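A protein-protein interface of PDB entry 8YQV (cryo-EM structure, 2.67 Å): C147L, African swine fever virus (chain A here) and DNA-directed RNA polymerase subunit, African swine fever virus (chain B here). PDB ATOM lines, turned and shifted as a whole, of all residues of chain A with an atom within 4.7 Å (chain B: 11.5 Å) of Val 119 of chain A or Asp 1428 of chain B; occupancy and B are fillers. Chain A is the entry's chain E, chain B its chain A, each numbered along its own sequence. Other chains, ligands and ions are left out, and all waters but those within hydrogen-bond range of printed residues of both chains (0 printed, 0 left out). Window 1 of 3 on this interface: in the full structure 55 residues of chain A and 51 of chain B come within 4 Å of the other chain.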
ATOM      1  N   LEU A  71      32.870  -0.492   8.630  1.00  0.00           N
ATOM      2  CA  LEU A  71      33.431  -0.453   9.970  1.00  0.00           C
ATOM      3  C   LEU A  71      34.788   0.229   9.942  1.00  0.00           C
ATOM      4  O   LEU A  71      35.593   0.002   9.039  1.00  0.00           O
ATOM      5  CB  LEU A  71      33.582  -1.869  10.521  1.00  0.00           C
ATOM      6  CG  LEU A  71      32.350  -2.616  11.012  1.00  0.00           C
ATOM      7  CD1 LEU A  71      32.583  -4.103  10.984  1.00  0.00           C
ATOM      8  CD2 LEU A  71      31.992  -2.161  12.403  1.00  0.00           C
ATOM      9  N   GLU A  75      36.327   0.183  15.239  1.00  0.00           N
ATOM     10  CA  GLU A  75      35.043  -0.452  15.519  1.00  0.00           C
ATOM     11  C   GLU A  75      35.110  -1.959  15.333  1.00  0.00           C
ATOM     12  O   GLU A  75      34.535  -2.708  16.127  1.00  0.00           O
ATOM     13  CB  GLU A  75      33.955   0.149  14.635  1.00  0.00           C
ATOM     14  CG  GLU A  75      33.511   1.518  15.076  1.00  0.00           C
ATOM     15  CD  GLU A  75      32.703   2.251  14.031  1.00  0.00           C
ATOM     16  OE1 GLU A  75      32.565   1.738  12.908  1.00  0.00           O
ATOM     17  OE2 GLU A  75      32.218   3.355  14.330  1.00  0.00           O
ATOM     18  N   LEU A  79      34.515  -4.637  18.282  1.00  0.00           N
ATOM     19  CA  LEU A  79      33.526  -5.702  18.164  1.00  0.00           C
ATOM     20  C   LEU A  79      34.152  -7.063  18.413  1.00  0.00           C
ATOM     21  O   LEU A  79      33.594  -7.887  19.144  1.00  0.00           O
ATOM     22  CB  LEU A  79      32.878  -5.681  16.784  1.00  0.00           C
ATOM     23  CG  LEU A  79      31.849  -4.626  16.415  1.00  0.00           C
ATOM     24  CD1 LEU A  79      31.650  -4.702  14.943  1.00  0.00           C
ATOM     25  CD2 LEU A  79      30.540  -4.852  17.116  1.00  0.00           C
ATOM     26  N   LEU A 117      26.148  -8.349  17.640  1.00  0.00           N
ATOM     27  CA  LEU A 117      26.338  -7.045  18.250  1.00  0.00           C
ATOM     28  C   LEU A 117      25.913  -5.966  17.269  1.00  0.00           C
ATOM     29  O   LEU A 117      25.819  -6.199  16.066  1.00  0.00           O
ATOM     30  CB  LEU A 117      27.794  -6.825  18.672  1.00  0.00           C
ATOM     31  CG  LEU A 117      28.406  -7.781  19.695  1.00  0.00           C
ATOM     32  CD1 LEU A 117      29.891  -7.534  19.816  1.00  0.00           C
ATOM     33  CD2 LEU A 117      27.749  -7.617  21.032  1.00  0.00           C
ATOM     34  N   LEU A 118      25.648  -4.777  17.802  1.00  0.00           N
ATOM     35  CA  LEU A 118      25.323  -3.608  17.001  1.00  0.00           C
ATOM     36  C   LEU A 118      26.251  -2.473  17.395  1.00  0.00           C
ATOM     37  O   LEU A 118      26.759  -2.433  18.515  1.00  0.00           O
ATOM     38  CB  LEU A 118      23.871  -3.174  17.188  1.00  0.00           C
ATOM     39  CG  LEU A 118      22.770  -4.144  16.778  1.00  0.00           C
ATOM     40  CD1 LEU A 118      21.444  -3.623  17.249  1.00  0.00           C
ATOM     41  CD2 LEU A 118      22.750  -4.340  15.289  1.00  0.00           C
ATOM     42  N   VAL A 119      26.474  -1.553  16.465  1.00  0.00           N
ATOM     43  CA  VAL A 119      27.361  -0.415  16.674  1.00  0.00           C
ATOM     44  C   VAL A 119      26.503   0.831  16.829  1.00  0.00           C
ATOM     45  O   VAL A 119      25.752   1.191  15.916  1.00  0.00           O
ATOM     46  CB  VAL A 119      28.356  -0.254  15.516  1.00  0.00           C
ATOM     47  CG1 VAL A 119      29.206   0.979  15.714  1.00  0.00           C
ATOM     48  CG2 VAL A 119      29.223  -1.484  15.394  1.00  0.00           C
ATOM     49  N   MET A 120      26.613   1.487  17.978  1.00  0.00           N
ATOM     50  CA  MET A 120      25.896   2.725  18.251  1.00  0.00           C
ATOM     51  C   MET A 120      26.848   3.901  18.093  1.00  0.00           C
ATOM     52  O   MET A 120      27.842   4.001  18.814  1.00  0.00           O
ATOM     53  CB  MET A 120      25.291   2.709  19.653  1.00  0.00           C
ATOM     54  CG  MET A 120      23.957   3.415  19.754  1.00  0.00           C
ATOM     55  SD  MET A 120      23.429   3.784  21.432  1.00  0.00           S
ATOM     56  CE  MET A 120      24.918   4.501  22.095  1.00  0.00           C
ATOM     57  N   ARG A 121      26.540   4.784  17.155  1.00  0.00           N
ATOM     58  CA  ARG A 121      27.343   5.967  16.879  1.00  0.00           C
ATOM     59  C   ARG A 121      26.595   7.178  17.418  1.00  0.00           C
ATOM     60  O   ARG A 121      25.578   7.585  16.853  1.00  0.00           O
ATOM     61  CB  ARG A 121      27.616   6.092  15.382  1.00  0.00           C
ATOM     62  CG  ARG A 121      28.649   5.109  14.868  1.00  0.00           C
ATOM     63  CD  ARG A 121      28.742   5.101  13.362  1.00  0.00           C
ATOM     64  NE  ARG A 121      29.853   4.286  12.889  1.00  0.00           N
ATOM     65  CZ  ARG A 121      29.975   3.821  11.655  1.00  0.00           C
ATOM     66  NH1 ARG A 121      29.070   4.072  10.731  1.00  0.00           N
ATOM     67  NH2 ARG A 121      31.033   3.083  11.342  1.00  0.00           N
ATOM     68  N   GLU A 134      23.071   6.724  15.733  1.00  0.00           N
ATOM     69  CA  GLU A 134      22.886   5.889  14.557  1.00  0.00           C
ATOM     70  C   GLU A 134      23.216   4.453  14.923  1.00  0.00           C
ATOM     71  O   GLU A 134      24.288   4.185  15.468  1.00  0.00           O
ATOM     72  CB  GLU A 134      23.776   6.340  13.405  1.00  0.00           C
ATOM     73  CG  GLU A 134      23.134   7.320  12.469  1.00  0.00           C
ATOM     74  CD  GLU A 134      24.150   8.102  11.685  1.00  0.00           C
ATOM     75  OE1 GLU A 134      25.348   7.800  11.816  1.00  0.00           O
ATOM     76  OE2 GLU A 134      23.761   9.019  10.939  1.00  0.00           O
ATOM     77  N   ILE A 135      22.304   3.537  14.618  1.00  0.00           N
ATOM     78  CA  ILE A 135      22.496   2.117  14.885  1.00  0.00           C
ATOM     79  C   ILE A 135      22.976   1.460  13.603  1.00  0.00           C
ATOM     80  O   ILE A 135      22.287   1.504  12.579  1.00  0.00           O
ATOM     81  CB  ILE A 135      21.207   1.452  15.382  1.00  0.00           C
ATOM     82  CG1 ILE A 135      20.713   2.115  16.662  1.00  0.00           C
ATOM     83  CG2 ILE A 135      21.446  -0.018  15.636  1.00  0.00           C
ATOM     84  CD1 ILE A 135      21.611   1.900  17.812  1.00  0.00           C
ATOM     85  N   TRP A 136      24.146   0.840  13.657  1.00  0.00           N
ATOM     86  CA  TRP A 136      24.753   0.215  12.495  1.00  0.00           C
ATOM     87  C   TRP A 136      24.925  -1.270  12.763  1.00  0.00           C
ATOM     88  O   TRP A 136      25.426  -1.659  13.819  1.00  0.00           O
ATOM     89  CB  TRP A 136      26.094   0.869  12.167  1.00  0.00           C
ATOM     90  CG  TRP A 136      25.970   2.147  11.400  1.00  0.00           C
ATOM     91  CD1 TRP A 136      26.017   3.404  11.907  1.00  0.00           C
ATOM     92  CD2 TRP A 136      25.778   2.291   9.990  1.00  0.00           C
ATOM     93  NE1 TRP A 136      25.868   4.323  10.906  1.00  0.00           N
ATOM     94  CE2 TRP A 136      25.719   3.662   9.718  1.00  0.00           C
ATOM     95  CE3 TRP A 136      25.648   1.391   8.932  1.00  0.00           C
ATOM     96  CZ2 TRP A 136      25.538   4.154   8.436  1.00  0.00           C
ATOM     97  CZ3 TRP A 136      25.474   1.882   7.667  1.00  0.00           C
ATOM     98  CH2 TRP A 136      25.418   3.248   7.427  1.00  0.00           C
ATOM     99  N   PRO A 138      26.781  -4.570  12.066  1.00  0.00           N
ATOM    100  CA  PRO A 138      28.026  -5.048  11.446  1.00  0.00           C
ATOM    101  C   PRO A 138      27.852  -6.256  10.549  1.00  0.00           C
ATOM    102  O   PRO A 138      28.752  -6.538   9.751  1.00  0.00           O
ATOM    103  CB  PRO A 138      28.913  -5.374  12.650  1.00  0.00           C
ATOM    104  CG  PRO A 138      27.986  -5.538  13.777  1.00  0.00           C
ATOM    105  CD  PRO A 138      26.851  -4.614  13.531  1.00  0.00           C
ATOM    106  N   TYR B   5      26.346   0.424  36.837  1.00  0.00           N
ATOM    107  CA  TYR B   5      27.507   0.963  36.148  1.00  0.00           C
ATOM    108  C   TYR B   5      27.274   2.415  35.758  1.00  0.00           C
ATOM    109  O   TYR B   5      26.237   2.755  35.183  1.00  0.00           O
ATOM    110  CB  TYR B   5      27.802   0.126  34.906  1.00  0.00           C
ATOM    111  CG  TYR B   5      28.902   0.664  34.029  1.00  0.00           C
ATOM    112  CD1 TYR B   5      30.224   0.393  34.299  1.00  0.00           C
ATOM    113  CD2 TYR B   5      28.611   1.444  32.929  1.00  0.00           C
ATOM    114  CE1 TYR B   5      31.220   0.880  33.497  1.00  0.00           C
ATOM    115  CE2 TYR B   5      29.598   1.936  32.128  1.00  0.00           C
ATOM    116  CZ  TYR B   5      30.899   1.653  32.413  1.00  0.00           C
ATOM    117  OH  TYR B   5      31.887   2.149  31.604  1.00  0.00           O
ATOM    118  N   ALA B   6      28.251   3.270  36.045  1.00  0.00           N
ATOM    119  CA  ALA B   6      28.145   4.684  35.734  1.00  0.00           C
ATOM    120  C   ALA B   6      29.467   5.185  35.176  1.00  0.00           C
ATOM    121  O   ALA B   6      30.504   4.531  35.290  1.00  0.00           O
ATOM    122  CB  ALA B   6      27.750   5.506  36.963  1.00  0.00           C
ATOM    123  N   GLU B   7      29.410   6.351  34.548  1.00  0.00           N
ATOM    124  CA  GLU B   7      30.589   7.055  34.075  1.00  0.00           C
ATOM    125  C   GLU B   7      30.458   8.521  34.439  1.00  0.00           C
ATOM    126  O   GLU B   7      29.362   9.080  34.391  1.00  0.00           O
ATOM    127  CB  GLU B   7      30.763   6.901  32.564  1.00  0.00           C
ATOM    128  CG  GLU B   7      31.132   5.497  32.136  1.00  0.00           C
ATOM    129  CD  GLU B   7      31.049   5.288  30.642  1.00  0.00           C
ATOM    130  OE1 GLU B   7      30.649   6.225  29.926  1.00  0.00           O
ATOM    131  OE2 GLU B   7      31.371   4.174  30.183  1.00  0.00           O
ATOM    132  N   MET B 472      40.478  -8.921  25.649  1.00  0.00           N
ATOM    133  CA  MET B 472      40.279  -7.681  24.908  1.00  0.00           C
ATOM    134  C   MET B 472      41.596  -7.005  24.569  1.00  0.00           C
ATOM    135  O   MET B 472      41.763  -6.490  23.461  1.00  0.00           O
ATOM    136  CB  MET B 472      39.395  -6.717  25.689  1.00  0.00           C
ATOM    137  CG  MET B 472      38.007  -7.200  25.964  1.00  0.00           C
ATOM    138  SD  MET B 472      36.932  -5.771  26.059  1.00  0.00           S
ATOM    139  CE  MET B 472      35.443  -6.515  26.659  1.00  0.00           C
ATOM    140  N   TYR B 840      32.329  11.775  13.674  1.00  0.00           N
ATOM    141  CA  TYR B 840      31.669  10.906  12.714  1.00  0.00           C
ATOM    142  C   TYR B 840      31.481  11.569  11.364  1.00  0.00           C
ATOM    143  O   TYR B 840      31.037  10.911  10.420  1.00  0.00           O
ATOM    144  CB  TYR B 840      30.320  10.446  13.260  1.00  0.00           C
ATOM    145  CG  TYR B 840      30.454   9.479  14.401  1.00  0.00           C
ATOM    146  CD1 TYR B 840      31.099   8.274  14.232  1.00  0.00           C
ATOM    147  CD2 TYR B 840      29.943   9.774  15.647  1.00  0.00           C
ATOM    148  CE1 TYR B 840      31.239   7.400  15.264  1.00  0.00           C
ATOM    149  CE2 TYR B 840      30.076   8.900  16.683  1.00  0.00           C
ATOM    150  CZ  TYR B 840      30.722   7.713  16.486  1.00  0.00           C
ATOM    151  OH  TYR B 840      30.856   6.828  17.522  1.00  0.00           O
ATOM    152  N   TYR B1037      37.012   7.290  12.460  1.00  0.00           N
ATOM    153  CA  TYR B1037      36.255   7.994  13.483  1.00  0.00           C
ATOM    154  C   TYR B1037      36.929   7.810  14.828  1.00  0.00           C
ATOM    155  O   TYR B1037      37.266   6.688  15.209  1.00  0.00           O
ATOM    156  CB  TYR B1037      34.834   7.453  13.550  1.00  0.00           C
ATOM    157  CG  TYR B1037      34.036   7.559  12.282  1.00  0.00           C
ATOM    158  CD1 TYR B1037      34.163   8.643  11.443  1.00  0.00           C
ATOM    159  CD2 TYR B1037      33.155   6.561  11.924  1.00  0.00           C
ATOM    160  CE1 TYR B1037      33.421   8.732  10.299  1.00  0.00           C
ATOM    161  CE2 TYR B1037      32.419   6.642  10.778  1.00  0.00           C
ATOM    162  CZ  TYR B1037      32.557   7.725   9.967  1.00  0.00           C
ATOM    163  OH  TYR B1037      31.815   7.808   8.819  1.00  0.00           O
ATOM    164  N   GLY B1038      37.104   8.894  15.565  1.00  0.00           N
ATOM    165  CA  GLY B1038      37.651   8.789  16.895  1.00  0.00           C
ATOM    166  C   GLY B1038      39.141   8.611  16.972  1.00  0.00           C
ATOM    167  O   GLY B1038      39.639   8.097  17.976  1.00  0.00           O
ATOM    168  N   VAL B1419      39.077   6.219  31.206  1.00  0.00           N
ATOM    169  CA  VAL B1419      39.828   6.115  29.960  1.00  0.00           C
ATOM    170  C   VAL B1419      39.214   7.054  28.928  1.00  0.00           C
ATOM    171  O   VAL B1419      37.995   7.270  28.935  1.00  0.00           O
ATOM    172  CB  VAL B1419      39.865   4.669  29.444  1.00  0.00           C
ATOM    173  CG1 VAL B1419      40.633   3.794  30.402  1.00  0.00           C
ATOM    174  CG2 VAL B1419      38.465   4.134  29.257  1.00  0.00           C
ATOM    175  N   PRO B1420      40.014   7.641  28.041  1.00  0.00           N
ATOM    176  CA  PRO B1420      39.456   8.514  27.006  1.00  0.00           C
ATOM    177  C   PRO B1420      38.513   7.777  26.067  1.00  0.00           C
ATOM    178  O   PRO B1420      38.728   6.617  25.719  1.00  0.00           O
ATOM    179  CB  PRO B1420      40.699   9.012  26.265  1.00  0.00           C
ATOM    180  CG  PRO B1420      41.791   8.878  27.240  1.00  0.00           C
ATOM    181  CD  PRO B1420      41.482   7.671  28.049  1.00  0.00           C
ATOM    182  N   ARG B1421      37.460   8.473  25.651  1.00  0.00           N
ATOM    183  CA  ARG B1421      36.533   7.962  24.645  1.00  0.00           C
ATOM    184  C   ARG B1421      37.149   8.234  23.278  1.00  0.00           C
ATOM    185  O   ARG B1421      36.890   9.243  22.623  1.00  0.00           O
ATOM    186  CB  ARG B1421      35.164   8.604  24.804  1.00  0.00           C
ATOM    187  CG  ARG B1421      34.172   8.239  23.732  1.00  0.00           C
ATOM    188  CD  ARG B1421      32.767   8.506  24.190  1.00  0.00           C
ATOM    189  NE  ARG B1421      32.612   8.227  25.610  1.00  0.00           N
ATOM    190  CZ  ARG B1421      31.446   8.182  26.238  1.00  0.00           C
ATOM    191  NH1 ARG B1421      30.312   8.417  25.604  1.00  0.00           N
ATOM    192  NH2 ARG B1421      31.420   7.896  27.536  1.00  0.00           N
ATOM    193  N   ILE B1422      37.989   7.299  22.849  1.00  0.00           N
ATOM    194  CA  ILE B1422      38.911   7.505  21.743  1.00  0.00           C
ATOM    195  C   ILE B1422      39.256   6.148  21.161  1.00  0.00           C
ATOM    196  O   ILE B1422      39.323   5.156  21.885  1.00  0.00           O
ATOM    197  CB  ILE B1422      40.166   8.256  22.234  1.00  0.00           C
ATOM    198  CG1 ILE B1422      39.970   9.749  22.103  1.00  0.00           C
ATOM    199  CG2 ILE B1422      41.421   7.831  21.511  1.00  0.00           C
ATOM    200  CD1 ILE B1422      41.060  10.482  22.726  1.00  0.00           C
ATOM    201  N   GLY B1423      39.454   6.097  19.852  1.00  0.00           N
ATOM    202  CA  GLY B1423      39.899   4.869  19.238  1.00  0.00           C
ATOM    203  C   GLY B1423      38.879   3.763  19.339  1.00  0.00           C
ATOM    204  O   GLY B1423      37.784   3.869  18.788  1.00  0.00           O
ATOM    205  N   THR B1424      39.228   2.691  20.049  1.00  0.00           N
ATOM    206  CA  THR B1424      38.322   1.557  20.171  1.00  0.00           C
ATOM    207  C   THR B1424      37.115   1.868  21.043  1.00  0.00           C
ATOM    208  O   THR B1424      36.121   1.142  20.980  1.00  0.00           O
ATOM    209  CB  THR B1424      39.071   0.342  20.714  1.00  0.00           C
ATOM    210  OG1 THR B1424      39.950   0.749  21.762  1.00  0.00           O
ATOM    211  CG2 THR B1424      39.881  -0.303  19.624  1.00  0.00           C
ATOM    212  N   MET B1425      37.166   2.933  21.835  1.00  0.00           N
ATOM    213  CA  MET B1425      36.073   3.306  22.717  1.00  0.00           C
ATOM    214  C   MET B1425      35.286   4.494  22.213  1.00  0.00           C
ATOM    215  O   MET B1425      34.483   5.048  22.963  1.00  0.00           O
ATOM    216  CB  MET B1425      36.607   3.600  24.108  1.00  0.00           C
ATOM    217  CG  MET B1425      37.565   2.559  24.535  1.00  0.00           C
ATOM    218  SD  MET B1425      36.761   1.168  25.298  1.00  0.00           S
ATOM    219  CE  MET B1425      38.008   0.808  26.492  1.00  0.00           C
ATOM    220  N   TYR B1426      35.500   4.905  20.969  1.00  0.00           N
ATOM    221  CA  TYR B1426      34.753   6.032  20.437  1.00  0.00           C
ATOM    222  C   TYR B1426      33.304   5.652  20.170  1.00  0.00           C
ATOM    223  O   TYR B1426      32.387   6.404  20.508  1.00  0.00           O
ATOM    224  CB  TYR B1426      35.428   6.558  19.171  1.00  0.00           C
ATOM    225  CG  TYR B1426      34.946   7.925  18.791  1.00  0.00           C
ATOM    226  CD1 TYR B1426      35.338   9.037  19.503  1.00  0.00           C
ATOM    227  CD2 TYR B1426      34.082   8.102  17.735  1.00  0.00           C
ATOM    228  CE1 TYR B1426      34.889  10.275  19.168  1.00  0.00           C
ATOM    229  CE2 TYR B1426      33.631   9.340  17.395  1.00  0.00           C
ATOM    230  CZ  TYR B1426      34.035  10.422  18.115  1.00  0.00           C
ATOM    231  OH  TYR B1426      33.584  11.671  17.780  1.00  0.00           O
ATOM    232  N   SER B1427      33.078   4.485  19.579  1.00  0.00           N
ATOM    233  CA  SER B1427      31.733   4.005  19.305  1.00  0.00           C
ATOM    234  C   SER B1427      31.280   3.053  20.399  1.00  0.00           C
ATOM    235  O   SER B1427      32.067   2.257  20.914  1.00  0.00           O
ATOM    236  CB  SER B1427      31.669   3.300  17.952  1.00  0.00           C
ATOM    237  OG  SER B1427      31.836   4.218  16.891  1.00  0.00           O
ATOM    238  N   ASP B1428      30.007   3.147  20.754  1.00  0.00           N
ATOM    239  CA  ASP B1428      29.415   2.299  21.775  1.00  0.00           C
ATOM    240  C   ASP B1428      28.885   1.028  21.132  1.00  0.00           C
ATOM    241  O   ASP B1428      28.348   1.059  20.025  1.00  0.00           O
ATOM    242  CB  ASP B1428      28.288   3.033  22.499  1.00  0.00           C
ATOM    243  CG  ASP B1428      28.086   2.542  23.920  1.00  0.00           C
ATOM    244  OD1 ASP B1428      28.593   1.453  24.262  1.00  0.00           O
ATOM    245  OD2 ASP B1428      27.416   3.248  24.701  1.00  0.00           O
ATOM    246  N   ILE B1429      29.049  -0.089  21.826  1.00  0.00           N
ATOM    247  CA  ILE B1429      28.532  -1.376  21.385  1.00  0.00           C
ATOM    248  C   ILE B1429      27.295  -1.695  22.207  1.00  0.00           C
ATOM    249  O   ILE B1429      27.285  -1.502  23.426  1.00  0.00           O
ATOM    250  CB  ILE B1429      29.591  -2.484  21.526  1.00  0.00           C
ATOM    251  CG1 ILE B1429      30.896  -2.083  20.837  1.00  0.00           C
ATOM    252  CG2 ILE B1429      29.080  -3.779  20.960  1.00  0.00           C
ATOM    253  CD1 ILE B1429      30.764  -1.796  19.367  1.00  0.00           C
ATOM    254  N   ILE B1430      26.241  -2.143  21.540  1.00  0.00           N
ATOM    255  CA  ILE B1430      25.043  -2.638  22.197  1.00  0.00           C
ATOM    256  C   ILE B1430      24.776  -4.040  21.677  1.00  0.00           C
ATOM    257  O   ILE B1430      25.231  -4.424  20.600  1.00  0.00           O
ATOM    258  CB  ILE B1430      23.823  -1.725  21.969  1.00  0.00           C
ATOM    259  CG1 ILE B1430      23.422  -1.718  20.501  1.00  0.00           C
ATOM    260  CG2 ILE B1430      24.125  -0.325  22.411  1.00  0.00           C
ATOM    261  CD1 ILE B1430      22.159  -0.980  20.239  1.00  0.00           C
ATOM    262  N   MET B1431      24.039  -4.814  22.461  1.00  0.00           N
ATOM    263  CA  MET B1431      23.794  -6.210  22.137  1.00  0.00           C
ATOM    264  C   MET B1431      22.603  -6.308  21.196  1.00  0.00           C
ATOM    265  O   MET B1431      21.563  -5.686  21.437  1.00  0.00           O
ATOM    266  CB  MET B1431      23.540  -7.017  23.409  1.00  0.00           C
ATOM    267  CG  MET B1431      24.725  -7.058  24.354  1.00  0.00           C
ATOM    268  SD  MET B1431      25.942  -8.344  24.066  1.00  0.00           S
ATOM    269  CE  MET B1431      24.989  -9.516  23.136  1.00  0.00           C
ATOM    270  N   ASP B1432      22.754  -7.085  20.128  1.00  0.00           N
ATOM    271  CA  ASP B1432      21.695  -7.253  19.135  1.00  0.00           C
ATOM    272  C   ASP B1432      20.645  -8.203  19.691  1.00  0.00           C
ATOM    273  O   ASP B1432      20.772  -9.422  19.578  1.00  0.00           O
ATOM    274  CB  ASP B1432      22.268  -7.770  17.825  1.00  0.00           C
ATOM    275  CG  ASP B1432      21.302  -7.629  16.672  1.00  0.00           C
ATOM    276  OD1 ASP B1432      20.141  -7.242  16.902  1.00  0.00           O
ATOM    277  OD2 ASP B1432      21.707  -7.893  15.524  1.00  0.00           O
ATOM    278  N   GLU B1433      19.595  -7.643  20.293  1.00  0.00           N
ATOM    279  CA  GLU B1433      18.550  -8.475  20.877  1.00  0.00           C
ATOM    280  C   GLU B1433      17.769  -9.220  19.805  1.00  0.00           C
ATOM    281  O   GLU B1433      17.502 -10.417  19.944  1.00  0.00           O
ATOM    282  CB  GLU B1433      17.607  -7.615  21.710  1.00  0.00           C
ATOM    283  CG  GLU B1433      18.294  -6.750  22.742  1.00  0.00           C
ATOM    284  CD  GLU B1433      17.350  -5.750  23.373  1.00  0.00           C
ATOM    285  OE1 GLU B1433      16.163  -5.729  22.987  1.00  0.00           O
ATOM    286  OE2 GLU B1433      17.791  -4.979  24.251  1.00  0.00           O
ATOM    287  N   TYR B1435      18.548 -10.341  17.003  1.00  0.00           N
ATOM    288  CA  TYR B1435      19.296 -11.437  16.406  1.00  0.00           C
ATOM    289  C   TYR B1435      19.532 -12.581  17.376  1.00  0.00           C
ATOM    290  O   TYR B1435      19.667 -13.730  16.947  1.00  0.00           O
ATOM    291  CB  TYR B1435      20.645 -10.926  15.899  1.00  0.00           C
ATOM    292  CG  TYR B1435      21.511 -11.956  15.223  1.00  0.00           C
ATOM    293  CD1 TYR B1435      21.185 -12.449  13.972  1.00  0.00           C
ATOM    294  CD2 TYR B1435      22.666 -12.419  15.827  1.00  0.00           C
ATOM    295  CE1 TYR B1435      21.980 -13.378  13.349  1.00  0.00           C
ATOM    296  CE2 TYR B1435      23.463 -13.350  15.213  1.00  0.00           C
ATOM    297  CZ  TYR B1435      23.116 -13.824  13.976  1.00  0.00           C
ATOM    298  OH  TYR B1435      23.912 -14.755  13.358  1.00  0.00           O
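The side-chain carboxylate (OE2) of Glu 75 of chain A is in hydrogen-bond range of the side-chain hydroxyl (OG) of Ser 1427 of chain B, at 2.7 Å. The backbone carbonyl oxygen (O) of Asp 1428 of chain B sits at hydrogen-bond distance from the backbone NH (N) of Met 120 of chain A (2.7 Å). O of Ile 1430 of chain B sits at hydrogen-bond distance from N of Leu 118 of chain A.
The side-chain hydroxyl (OH) of Tyr 840 of chain B sits at hydrogen-bond distance from the backbone carbonyl oxygen (O) of Tyr 1426 of chain B, 3.4 Å away. The backbone NH of Arg 121 of chain A is in hydrogen-bond range of the backbone carbonyl oxygen of Glu 134 of chain A (2.9 Å). The backbone NH of Tyr 1435 of chain B is in hydrogen-bond range of the side-chain carboxylate of Asp 1432 of chain B. The backbone carbonyl oxygen (O) of Val 119 of chain A is in hydrogen-bond range of the backbone NH (N) of Trp 136 of chain A, 2.8 Å away. The side-chain hydroxyl (OH) of Tyr 840 of chain B is in hydrogen-bond range of the side-chain hydroxyl (OG) of Ser 1427 of chain B, 2.9 Å away. The side-chain carboxylate (OE1) of Glu 75 of chain A lies within salt-bridge range of the guanidinium group (NH2) of Arg 121 of chain A (2.6 Å).
Leu 79 of chain A touches Ile 1429 of chain B (CD2 to CD1, 3.8 Å). Leu 117 of chain A touches Met 1431 of chain B (CD2 to SD, 3.6 Å). Asp 1432 of chain B touches Leu 117 of chain A. Ile 1429 of chain B touches Leu 118 of chain A (CA to O, 3.5 Å). Leu 118 of chain A touches Asp 1432 of chain B (CD2 to OD2, 3.7 Å). Asp 1428 of chain B touches Val 119 of chain A (O to C, 3.7 Å). Met 120 of chain A touches Ser 1427 of chain B. Arg 121 of chain A touches Tyr 1037 of chain B. Arg 121 of chain A touches Ser 1427 of chain B. CD1 of Ile 135 of chain A touches CD1 of Ile 1430 of chain B (3.8 Å).
Printed residues of chain B within 4 Å of Glu 75 of chain A: Ser 1427 (2.7 Å). Printed residues of chain B within 4 Å of Leu 117 of chain A: Ile 1430, Met 1431 and Asp 1432. Printed residues of chain B within 4 Å of Val 119 of chain A: Asp 1428. Of the printed residues of chain B, Arg 121 of chain A touches Tyr 840 (3.5 Å), Tyr 1037 (3.8 Å) and Ser 1427 (3.9 Å). Ala 6 of chain B touches none of the printed residues of chain A. Of the printed residues of chain A, Tyr 1037 of chain B touches Arg 121. Asp 1428 of chain B touches just these residues of chain A: Val 119 and Met 120. Printed residues of chain A within 4 Å of Ile 1429 of chain B: Leu 79 (3.8 Å) and Leu 118 (3.5 Å). Of the printed residues of chain A, Asp 1432 of chain B touches Leu 117 (3.9 Å) and Leu 118 (3.7 Å). The nearest residue of chain B that does not touch Val 119 of chain A is Ser 1427 of chain B (4.1 Å).
Of the 23 printed residues of chain B, 8 touch a printed residue of chain A. Printed residues of chain A that touch a printed residue of chain B: Glu 75, Leu 79, Leu 117, Leu 118, Val 119, Met 120, Arg 121 and Ile 135. Hydrophobic or aromatic side chains of chain A within 4 Å of the printed part of chain B: Leu 79, Leu 117, Leu 118, Met 120 and Ile 135. Among the printed residues, 15 pairs touch across the chains. Among the printed residues, no Asp or Glu carboxylate lies within 4 Å of a Lys or Arg side-chain nitrogen of the other chain.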
